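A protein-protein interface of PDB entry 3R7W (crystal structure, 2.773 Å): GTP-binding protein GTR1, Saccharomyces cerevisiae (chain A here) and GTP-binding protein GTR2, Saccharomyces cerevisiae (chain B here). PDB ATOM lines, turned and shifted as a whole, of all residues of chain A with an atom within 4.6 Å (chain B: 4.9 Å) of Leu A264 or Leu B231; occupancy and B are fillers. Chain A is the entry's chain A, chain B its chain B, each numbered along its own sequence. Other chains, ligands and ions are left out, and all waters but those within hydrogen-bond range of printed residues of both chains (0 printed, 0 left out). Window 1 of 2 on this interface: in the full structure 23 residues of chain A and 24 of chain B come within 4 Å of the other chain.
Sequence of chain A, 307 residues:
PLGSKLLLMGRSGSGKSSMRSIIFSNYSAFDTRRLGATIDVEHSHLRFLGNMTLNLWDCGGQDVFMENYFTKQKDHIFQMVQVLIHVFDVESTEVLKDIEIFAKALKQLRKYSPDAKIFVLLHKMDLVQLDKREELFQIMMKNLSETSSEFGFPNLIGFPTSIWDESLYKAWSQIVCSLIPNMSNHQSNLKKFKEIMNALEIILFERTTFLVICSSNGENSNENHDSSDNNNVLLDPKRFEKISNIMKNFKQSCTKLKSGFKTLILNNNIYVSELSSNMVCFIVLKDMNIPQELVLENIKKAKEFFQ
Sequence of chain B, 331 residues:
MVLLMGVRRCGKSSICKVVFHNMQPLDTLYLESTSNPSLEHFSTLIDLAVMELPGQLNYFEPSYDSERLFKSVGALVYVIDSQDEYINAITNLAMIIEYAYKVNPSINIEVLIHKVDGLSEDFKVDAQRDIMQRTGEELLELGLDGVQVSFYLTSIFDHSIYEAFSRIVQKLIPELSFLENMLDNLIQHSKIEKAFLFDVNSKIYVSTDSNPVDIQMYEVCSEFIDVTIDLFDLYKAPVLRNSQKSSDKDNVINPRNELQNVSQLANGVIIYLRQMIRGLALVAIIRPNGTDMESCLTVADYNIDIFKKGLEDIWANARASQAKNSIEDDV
Of the printed residues of chain B, Ile A246 touches Val B227, Asp B230 and Leu B231.
Of the printed residues of chain B, Ile A265 touches Asn B261 and Val B262.
Printed residues of chain B within 4 Å of Ile A270: Tyr B235.
Of the printed residues of chain A, Leu B231 touches Ile A246, Met A247, Leu A264 and Phe A282.
Printed residues of chain A within 4 Å of Val B262: Leu A264 (3.3 Å) and Ile A265 (2.8 Å).
OG of Ser B263 sits at hydrogen-bond distance from O of Thr A263, 2.8 Å away.
OD1 of Asn B261 lies close to O of Ile A265 (2.7 Å).
The backbone carbonyl oxygen (O) of Val B262 is in hydrogen-bond range of the backbone NH (N) of Ile A265, 2.8 Å away.
Of the 13 printed residues of chain B, 10 touch a printed residue of chain A.
Hydrophobic or aromatic side chains of chain B within 4 Å of the printed part of chain A: Val B227, Leu B231, Leu B234 and Tyr B235.
Of the 12 printed residues of chain A, 9 touch a printed residue of chain B.
Hydrophobic or aromatic side chains of chain A that line the printed part of chain B: Ile A243, Ile A246, Met A247, Leu A264, Leu A266, Ile A270 and Phe A282.
N of Val A272 lies within hydrogen-bond range of O of Leu A264 (2.8 Å).
Leu B234 touches Ile A243 (CD2 to CG1, 3.5 Å).
CG2 of Ile A246 touches CG1 of Val B227, 3.97 Å away.
Asp B230 touches Ile A246 (CB to CD1, 3.8 Å).
CG2 of Ile A246 touches CD2 of Leu B231, at 3.9 Å.
CE of Met A247 touches CD1 of Leu B231 (3.1 Å).
Leu A264 touches Val B262 (CA to O, 3.3 Å).
Ser B263 touches Leu A264 (CB to CB, 3.7 Å).
Thr B228 touches Leu A266.
N of Phe B232 touches CD2 of Leu A266 (3.7 Å).
Leu A266 touches Asn B261 (CB to OD1, 3.1 Å).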
ATOM      1  N   ILE A 243     -18.463 -18.955 -20.514  1.00  0.00           N
ATOM      2  CA  ILE A 243     -17.178 -19.638 -20.339  1.00  0.00           C
ATOM      3  C   ILE A 243     -17.251 -20.611 -19.168  1.00  0.00           C
ATOM      4  O   ILE A 243     -16.677 -21.698 -19.229  1.00  0.00           O
ATOM      5  CB  ILE A 243     -16.005 -18.688 -20.157  1.00  0.00           C
ATOM      6  CG1 ILE A 243     -15.597 -18.083 -21.495  1.00  0.00           C
ATOM      7  CG2 ILE A 243     -14.843 -19.427 -19.593  1.00  0.00           C
ATOM      8  CD1 ILE A 243     -15.103 -16.665 -21.342  1.00  0.00           C
ATOM      9  N   ILE A 246     -19.129 -23.589 -20.920  1.00  0.00           N
ATOM     10  CA  ILE A 246     -18.273 -24.275 -21.868  1.00  0.00           C
ATOM     11  C   ILE A 246     -17.170 -25.051 -21.159  1.00  0.00           C
ATOM     12  O   ILE A 246     -16.896 -26.225 -21.471  1.00  0.00           O
ATOM     13  CB  ILE A 246     -17.609 -23.258 -22.726  1.00  0.00           C
ATOM     14  CG1 ILE A 246     -18.675 -22.536 -23.545  1.00  0.00           C
ATOM     15  CG2 ILE A 246     -16.556 -23.933 -23.569  1.00  0.00           C
ATOM     16  CD1 ILE A 246     -18.210 -21.267 -24.203  1.00  0.00           C
ATOM     17  N   MET A 247     -16.541 -24.385 -20.195  1.00  0.00           N
ATOM     18  CA  MET A 247     -15.514 -25.020 -19.398  1.00  0.00           C
ATOM     19  C   MET A 247     -16.045 -26.201 -18.609  1.00  0.00           C
ATOM     20  O   MET A 247     -15.411 -27.242 -18.588  1.00  0.00           O
ATOM     21  CB  MET A 247     -14.836 -24.015 -18.471  1.00  0.00           C
ATOM     22  CG  MET A 247     -13.720 -23.195 -19.140  1.00  0.00           C
ATOM     23  SD  MET A 247     -12.569 -24.226 -20.394  1.00  0.00           S
ATOM     24  CE  MET A 247     -13.117 -23.181 -21.916  1.00  0.00           C
ATOM     25  N   PHE A 261      -8.639 -31.545 -16.722  1.00  0.00           N
ATOM     26  CA  PHE A 261      -8.139 -30.453 -17.543  1.00  0.00           C
ATOM     27  C   PHE A 261      -7.039 -29.732 -16.767  1.00  0.00           C
ATOM     28  O   PHE A 261      -7.158 -29.554 -15.556  1.00  0.00           O
ATOM     29  CB  PHE A 261      -9.291 -29.501 -17.871  1.00  0.00           C
ATOM     30  CG  PHE A 261      -8.870 -28.081 -18.059  1.00  0.00           C
ATOM     31  CD1 PHE A 261      -8.743 -27.240 -16.973  1.00  0.00           C
ATOM     32  CD2 PHE A 261      -8.611 -27.591 -19.314  1.00  0.00           C
ATOM     33  CE1 PHE A 261      -8.356 -25.938 -17.129  1.00  0.00           C
ATOM     34  CE2 PHE A 261      -8.237 -26.290 -19.478  1.00  0.00           C
ATOM     35  CZ  PHE A 261      -8.109 -25.455 -18.379  1.00  0.00           C
ATOM     36  N   THR A 263      -4.273 -27.472 -18.893  1.00  0.00           N
ATOM     37  CA  THR A 263      -4.167 -26.258 -19.710  1.00  0.00           C
ATOM     38  C   THR A 263      -4.943 -26.332 -21.031  1.00  0.00           C
ATOM     39  O   THR A 263      -5.194 -27.416 -21.549  1.00  0.00           O
ATOM     40  CB  THR A 263      -2.668 -25.904 -20.042  1.00  0.00           C
ATOM     41  OG1 THR A 263      -2.122 -26.843 -20.982  1.00  0.00           O
ATOM     42  CG2 THR A 263      -1.815 -25.889 -18.781  1.00  0.00           C
ATOM     43  N   LEU A 264      -5.300 -25.179 -21.590  1.00  0.00           N
ATOM     44  CA  LEU A 264      -5.754 -25.131 -22.984  1.00  0.00           C
ATOM     45  C   LEU A 264      -5.301 -23.817 -23.608  1.00  0.00           C
ATOM     46  O   LEU A 264      -5.343 -22.792 -22.963  1.00  0.00           O
ATOM     47  CB  LEU A 264      -7.289 -25.362 -23.132  1.00  0.00           C
ATOM     48  CG  LEU A 264      -8.304 -24.272 -23.549  1.00  0.00           C
ATOM     49  CD1 LEU A 264      -7.927 -23.494 -24.788  1.00  0.00           C
ATOM     50  CD2 LEU A 264      -9.696 -24.857 -23.750  1.00  0.00           C
ATOM     51  N   ILE A 265      -4.859 -23.844 -24.856  1.00  0.00           N
ATOM     52  CA  ILE A 265      -4.465 -22.625 -25.550  1.00  0.00           C
ATOM     53  C   ILE A 265      -5.188 -22.647 -26.877  1.00  0.00           C
ATOM     54  O   ILE A 265      -5.247 -23.679 -27.523  1.00  0.00           O
ATOM     55  CB  ILE A 265      -2.915 -22.588 -25.769  1.00  0.00           C
ATOM     56  CG1 ILE A 265      -2.184 -22.702 -24.428  1.00  0.00           C
ATOM     57  CG2 ILE A 265      -2.476 -21.326 -26.501  1.00  0.00           C
ATOM     58  CD1 ILE A 265      -0.759 -23.185 -24.548  1.00  0.00           C
ATOM     59  N   LEU A 266      -5.745 -21.533 -27.302  1.00  0.00           N
ATOM     60  CA  LEU A 266      -6.531 -21.566 -28.521  1.00  0.00           C
ATOM     61  C   LEU A 266      -6.081 -20.483 -29.466  1.00  0.00           C
ATOM     62  O   LEU A 266      -6.092 -19.307 -29.124  1.00  0.00           O
ATOM     63  CB  LEU A 266      -8.012 -21.408 -28.204  1.00  0.00           C
ATOM     64  CG  LEU A 266      -8.969 -21.308 -29.384  1.00  0.00           C
ATOM     65  CD1 LEU A 266      -9.135 -22.667 -30.051  1.00  0.00           C
ATOM     66  CD2 LEU A 266     -10.298 -20.802 -28.860  1.00  0.00           C
ATOM     67  N   ILE A 270      -5.825 -17.377 -26.704  1.00  0.00           N
ATOM     68  CA  ILE A 270      -6.475 -17.637 -25.420  1.00  0.00           C
ATOM     69  C   ILE A 270      -5.656 -18.642 -24.650  1.00  0.00           C
ATOM     70  O   ILE A 270      -5.294 -19.679 -25.188  1.00  0.00           O
ATOM     71  CB  ILE A 270      -7.908 -18.265 -25.626  1.00  0.00           C
ATOM     72  CG1 ILE A 270      -8.657 -17.601 -26.795  1.00  0.00           C
ATOM     73  CG2 ILE A 270      -8.707 -18.295 -24.331  1.00  0.00           C
ATOM     74  CD1 ILE A 270     -10.003 -17.049 -26.472  1.00  0.00           C
ATOM     75  N   TYR A 271      -5.374 -18.375 -23.389  1.00  0.00           N
ATOM     76  CA  TYR A 271      -4.672 -19.358 -22.585  1.00  0.00           C
ATOM     77  C   TYR A 271      -5.454 -19.564 -21.324  1.00  0.00           C
ATOM     78  O   TYR A 271      -5.875 -18.605 -20.703  1.00  0.00           O
ATOM     79  CB  TYR A 271      -3.267 -18.873 -22.220  1.00  0.00           C
ATOM     80  CG  TYR A 271      -2.312 -18.723 -23.393  1.00  0.00           C
ATOM     81  CD1 TYR A 271      -1.154 -19.511 -23.491  1.00  0.00           C
ATOM     82  CD2 TYR A 271      -2.561 -17.792 -24.398  1.00  0.00           C
ATOM     83  CE1 TYR A 271      -0.279 -19.370 -24.563  1.00  0.00           C
ATOM     84  CE2 TYR A 271      -1.699 -17.646 -25.467  1.00  0.00           C
ATOM     85  CZ  TYR A 271      -0.559 -18.431 -25.546  1.00  0.00           C
ATOM     86  OH  TYR A 271       0.280 -18.254 -26.622  1.00  0.00           O
ATOM     87  N   VAL A 272      -5.640 -20.813 -20.935  1.00  0.00           N
ATOM     88  CA  VAL A 272      -6.395 -21.156 -19.752  1.00  0.00           C
ATOM     89  C   VAL A 272      -5.535 -22.143 -19.018  1.00  0.00           C
ATOM     90  O   VAL A 272      -5.054 -23.101 -19.615  1.00  0.00           O
ATOM     91  CB  VAL A 272      -7.695 -21.848 -20.138  1.00  0.00           C
ATOM     92  CG1 VAL A 272      -8.587 -22.037 -18.919  1.00  0.00           C
ATOM     93  CG2 VAL A 272      -8.421 -21.043 -21.215  1.00  0.00           C
ATOM     94  N   PHE A 282      -8.407 -17.343 -17.245  1.00  0.00           N
ATOM     95  CA  PHE A 282      -8.728 -17.318 -18.650  1.00  0.00           C
ATOM     96  C   PHE A 282      -8.139 -16.030 -19.178  1.00  0.00           C
ATOM     97  O   PHE A 282      -8.659 -14.956 -18.885  1.00  0.00           O
ATOM     98  CB  PHE A 282     -10.240 -17.322 -18.793  1.00  0.00           C
ATOM     99  CG  PHE A 282     -10.748 -17.477 -20.203  1.00  0.00           C
ATOM    100  CD1 PHE A 282     -11.133 -18.722 -20.682  1.00  0.00           C
ATOM    101  CD2 PHE A 282     -10.918 -16.370 -21.020  1.00  0.00           C
ATOM    102  CE1 PHE A 282     -11.642 -18.866 -21.969  1.00  0.00           C
ATOM    103  CE2 PHE A 282     -11.436 -16.505 -22.310  1.00  0.00           C
ATOM    104  CZ  PHE A 282     -11.792 -17.755 -22.783  1.00  0.00           C
ATOM    105  N   ASP B 226     -16.364 -28.598 -30.122  1.00  0.00           N
ATOM    106  CA  ASP B 226     -17.343 -27.660 -29.585  1.00  0.00           C
ATOM    107  C   ASP B 226     -16.686 -26.618 -28.698  1.00  0.00           C
ATOM    108  O   ASP B 226     -16.788 -25.409 -28.950  1.00  0.00           O
ATOM    109  CB  ASP B 226     -18.439 -28.395 -28.823  1.00  0.00           C
ATOM    110  CG  ASP B 226     -19.459 -29.021 -29.742  1.00  0.00           C
ATOM    111  OD1 ASP B 226     -19.538 -28.575 -30.930  1.00  0.00           O
ATOM    112  OD2 ASP B 226     -20.165 -29.947 -29.264  1.00  0.00           O
ATOM    113  N   VAL B 227     -16.000 -27.098 -27.667  1.00  0.00           N
ATOM    114  CA  VAL B 227     -15.208 -26.233 -26.804  1.00  0.00           C
ATOM    115  C   VAL B 227     -14.302 -25.249 -27.584  1.00  0.00           C
ATOM    116  O   VAL B 227     -14.296 -24.044 -27.273  1.00  0.00           O
ATOM    117  CB  VAL B 227     -14.425 -27.076 -25.784  1.00  0.00           C
ATOM    118  CG1 VAL B 227     -13.586 -26.205 -24.891  1.00  0.00           C
ATOM    119  CG2 VAL B 227     -15.436 -27.889 -24.953  1.00  0.00           C
ATOM    120  N   THR B 228     -13.577 -25.721 -28.608  1.00  0.00           N
ATOM    121  CA  THR B 228     -12.839 -24.768 -29.440  1.00  0.00           C
ATOM    122  C   THR B 228     -13.727 -23.807 -30.234  1.00  0.00           C
ATOM    123  O   THR B 228     -13.453 -22.602 -30.284  1.00  0.00           O
ATOM    124  CB  THR B 228     -11.747 -25.406 -30.369  1.00  0.00           C
ATOM    125  OG1 THR B 228     -11.755 -24.747 -31.645  1.00  0.00           O
ATOM    126  CG2 THR B 228     -11.960 -26.878 -30.569  1.00  0.00           C
ATOM    127  N   ILE B 229     -14.797 -24.319 -30.838  1.00  0.00           N
ATOM    128  CA  ILE B 229     -15.642 -23.455 -31.661  1.00  0.00           C
ATOM    129  C   ILE B 229     -16.424 -22.393 -30.872  1.00  0.00           C
ATOM    130  O   ILE B 229     -16.467 -21.233 -31.279  1.00  0.00           O
ATOM    131  CB  ILE B 229     -16.578 -24.259 -32.569  1.00  0.00           C
ATOM    132  CG1 ILE B 229     -15.756 -24.945 -33.673  1.00  0.00           C
ATOM    133  CG2 ILE B 229     -17.662 -23.343 -33.153  1.00  0.00           C
ATOM    134  CD1 ILE B 229     -16.555 -25.280 -34.938  1.00  0.00           C
ATOM    135  N   ASP B 230     -17.017 -22.800 -29.746  1.00  0.00           N
ATOM    136  CA  ASP B 230     -17.739 -21.893 -28.840  1.00  0.00           C
ATOM    137  C   ASP B 230     -16.858 -20.832 -28.165  1.00  0.00           C
ATOM    138  O   ASP B 230     -17.302 -19.711 -27.934  1.00  0.00           O
ATOM    139  CB  ASP B 230     -18.458 -22.673 -27.731  1.00  0.00           C
ATOM    140  CG  ASP B 230     -19.466 -23.701 -28.266  1.00  0.00           C
ATOM    141  OD1 ASP B 230     -20.023 -23.469 -29.370  1.00  0.00           O
ATOM    142  OD2 ASP B 230     -19.703 -24.725 -27.564  1.00  0.00           O
ATOM    143  N   LEU B 231     -15.625 -21.184 -27.806  1.00  0.00           N
ATOM    144  CA  LEU B 231     -14.752 -20.222 -27.143  1.00  0.00           C
ATOM    145  C   LEU B 231     -14.277 -19.196 -28.148  1.00  0.00           C
ATOM    146  O   LEU B 231     -14.301 -17.991 -27.902  1.00  0.00           O
ATOM    147  CB  LEU B 231     -13.557 -20.923 -26.524  1.00  0.00           C
ATOM    148  CG  LEU B 231     -13.761 -21.718 -25.246  1.00  0.00           C
ATOM    149  CD1 LEU B 231     -12.440 -22.297 -24.805  1.00  0.00           C
ATOM    150  CD2 LEU B 231     -14.336 -20.807 -24.184  1.00  0.00           C
ATOM    151  N   PHE B 232     -13.847 -19.703 -29.294  1.00  0.00           N
ATOM    152  CA  PHE B 232     -13.402 -18.871 -30.383  1.00  0.00           C
ATOM    153  C   PHE B 232     -14.486 -17.854 -30.664  1.00  0.00           C
ATOM    154  O   PHE B 232     -14.213 -16.656 -30.758  1.00  0.00           O
ATOM    155  CB  PHE B 232     -13.154 -19.734 -31.618  1.00  0.00           C
ATOM    156  CG  PHE B 232     -12.916 -18.945 -32.879  1.00  0.00           C
ATOM    157  CD1 PHE B 232     -13.951 -18.232 -33.480  1.00  0.00           C
ATOM    158  CD2 PHE B 232     -11.668 -18.933 -33.477  1.00  0.00           C
ATOM    159  CE1 PHE B 232     -13.743 -17.509 -34.638  1.00  0.00           C
ATOM    160  CE2 PHE B 232     -11.455 -18.219 -34.638  1.00  0.00           C
ATOM    161  CZ  PHE B 232     -12.496 -17.506 -35.219  1.00  0.00           C
ATOM    162  N   ASP B 233     -15.724 -18.328 -30.786  1.00  0.00           N
ATOM    163  CA  ASP B 233     -16.820 -17.457 -31.199  1.00  0.00           C
ATOM    164  C   ASP B 233     -17.170 -16.378 -30.171  1.00  0.00           C
ATOM    165  O   ASP B 233     -17.990 -15.494 -30.451  1.00  0.00           O
ATOM    166  CB  ASP B 233     -18.058 -18.271 -31.602  1.00  0.00           C
ATOM    167  CG  ASP B 233     -17.989 -18.760 -33.047  1.00  0.00           C
ATOM    168  OD1 ASP B 233     -17.545 -17.970 -33.917  1.00  0.00           O
ATOM    169  OD2 ASP B 233     -18.369 -19.930 -33.313  1.00  0.00           O
ATOM    170  N   LEU B 234     -16.557 -16.445 -28.990  1.00  0.00           N
ATOM    171  CA  LEU B 234     -16.860 -15.466 -27.942  1.00  0.00           C
ATOM    172  C   LEU B 234     -16.031 -14.209 -28.157  1.00  0.00           C
ATOM    173  O   LEU B 234     -16.377 -13.128 -27.668  1.00  0.00           O
ATOM    174  CB  LEU B 234     -16.610 -16.057 -26.545  1.00  0.00           C
ATOM    175  CG  LEU B 234     -17.769 -16.273 -25.563  1.00  0.00           C
ATOM    176  CD1 LEU B 234     -19.002 -16.802 -26.269  1.00  0.00           C
ATOM    177  CD2 LEU B 234     -17.347 -17.224 -24.442  1.00  0.00           C
ATOM    178  N   TYR B 235     -14.945 -14.366 -28.909  1.00  0.00           N
ATOM    179  CA  TYR B 235     -13.963 -13.302 -29.112  1.00  0.00           C
ATOM    180  C   TYR B 235     -13.494 -13.260 -30.578  1.00  0.00           C
ATOM    181  O   TYR B 235     -12.363 -13.658 -30.877  1.00  0.00           O
ATOM    182  CB  TYR B 235     -12.742 -13.524 -28.197  1.00  0.00           C
ATOM    183  CG  TYR B 235     -13.000 -13.453 -26.697  1.00  0.00           C
ATOM    184  CD1 TYR B 235     -13.122 -14.609 -25.930  1.00  0.00           C
ATOM    185  CD2 TYR B 235     -13.093 -12.233 -26.044  1.00  0.00           C
ATOM    186  CE1 TYR B 235     -13.349 -14.547 -24.544  1.00  0.00           C
ATOM    187  CE2 TYR B 235     -13.315 -12.163 -24.669  1.00  0.00           C
ATOM    188  CZ  TYR B 235     -13.445 -13.321 -23.924  1.00  0.00           C
ATOM    189  OH  TYR B 235     -13.665 -13.233 -22.560  1.00  0.00           O
ATOM    190  N   ASN B 261      -6.299 -25.757 -31.401  1.00  0.00           N
ATOM    191  CA  ASN B 261      -6.486 -25.759 -29.987  1.00  0.00           C
ATOM    192  C   ASN B 261      -5.648 -26.868 -29.475  1.00  0.00           C
ATOM    193  O   ASN B 261      -5.730 -27.995 -29.959  1.00  0.00           O
ATOM    194  CB  ASN B 261      -7.934 -26.084 -29.679  1.00  0.00           C
ATOM    195  CG  ASN B 261      -8.418 -25.430 -28.415  1.00  0.00           C
ATOM    196  OD1 ASN B 261      -7.816 -24.466 -27.931  1.00  0.00           O
ATOM    197  ND2 ASN B 261      -9.521 -25.934 -27.877  1.00  0.00           N
ATOM    198  N   VAL B 262      -4.815 -26.552 -28.501  1.00  0.00           N
ATOM    199  CA  VAL B 262      -4.079 -27.576 -27.808  1.00  0.00           C
ATOM    200  C   VAL B 262      -4.604 -27.580 -26.411  1.00  0.00           C
ATOM    201  O   VAL B 262      -4.813 -26.518 -25.820  1.00  0.00           O
ATOM    202  CB  VAL B 262      -2.617 -27.217 -27.641  1.00  0.00           C
ATOM    203  CG1 VAL B 262      -1.884 -28.427 -27.100  1.00  0.00           C
ATOM    204  CG2 VAL B 262      -2.029 -26.726 -28.943  1.00  0.00           C
ATOM    205  N   SER B 263      -4.776 -28.763 -25.847  1.00  0.00           N
ATOM    206  CA  SER B 263      -5.085 -28.804 -24.438  1.00  0.00           C
ATOM    207  C   SER B 263      -4.433 -30.009 -23.780  1.00  0.00           C
ATOM    208  O   SER B 263      -4.221 -31.036 -24.409  1.00  0.00           O
ATOM    209  CB  SER B 263      -6.593 -28.787 -24.236  1.00  0.00           C
ATOM    210  OG  SER B 263      -6.917 -29.187 -22.926  1.00  0.00           O
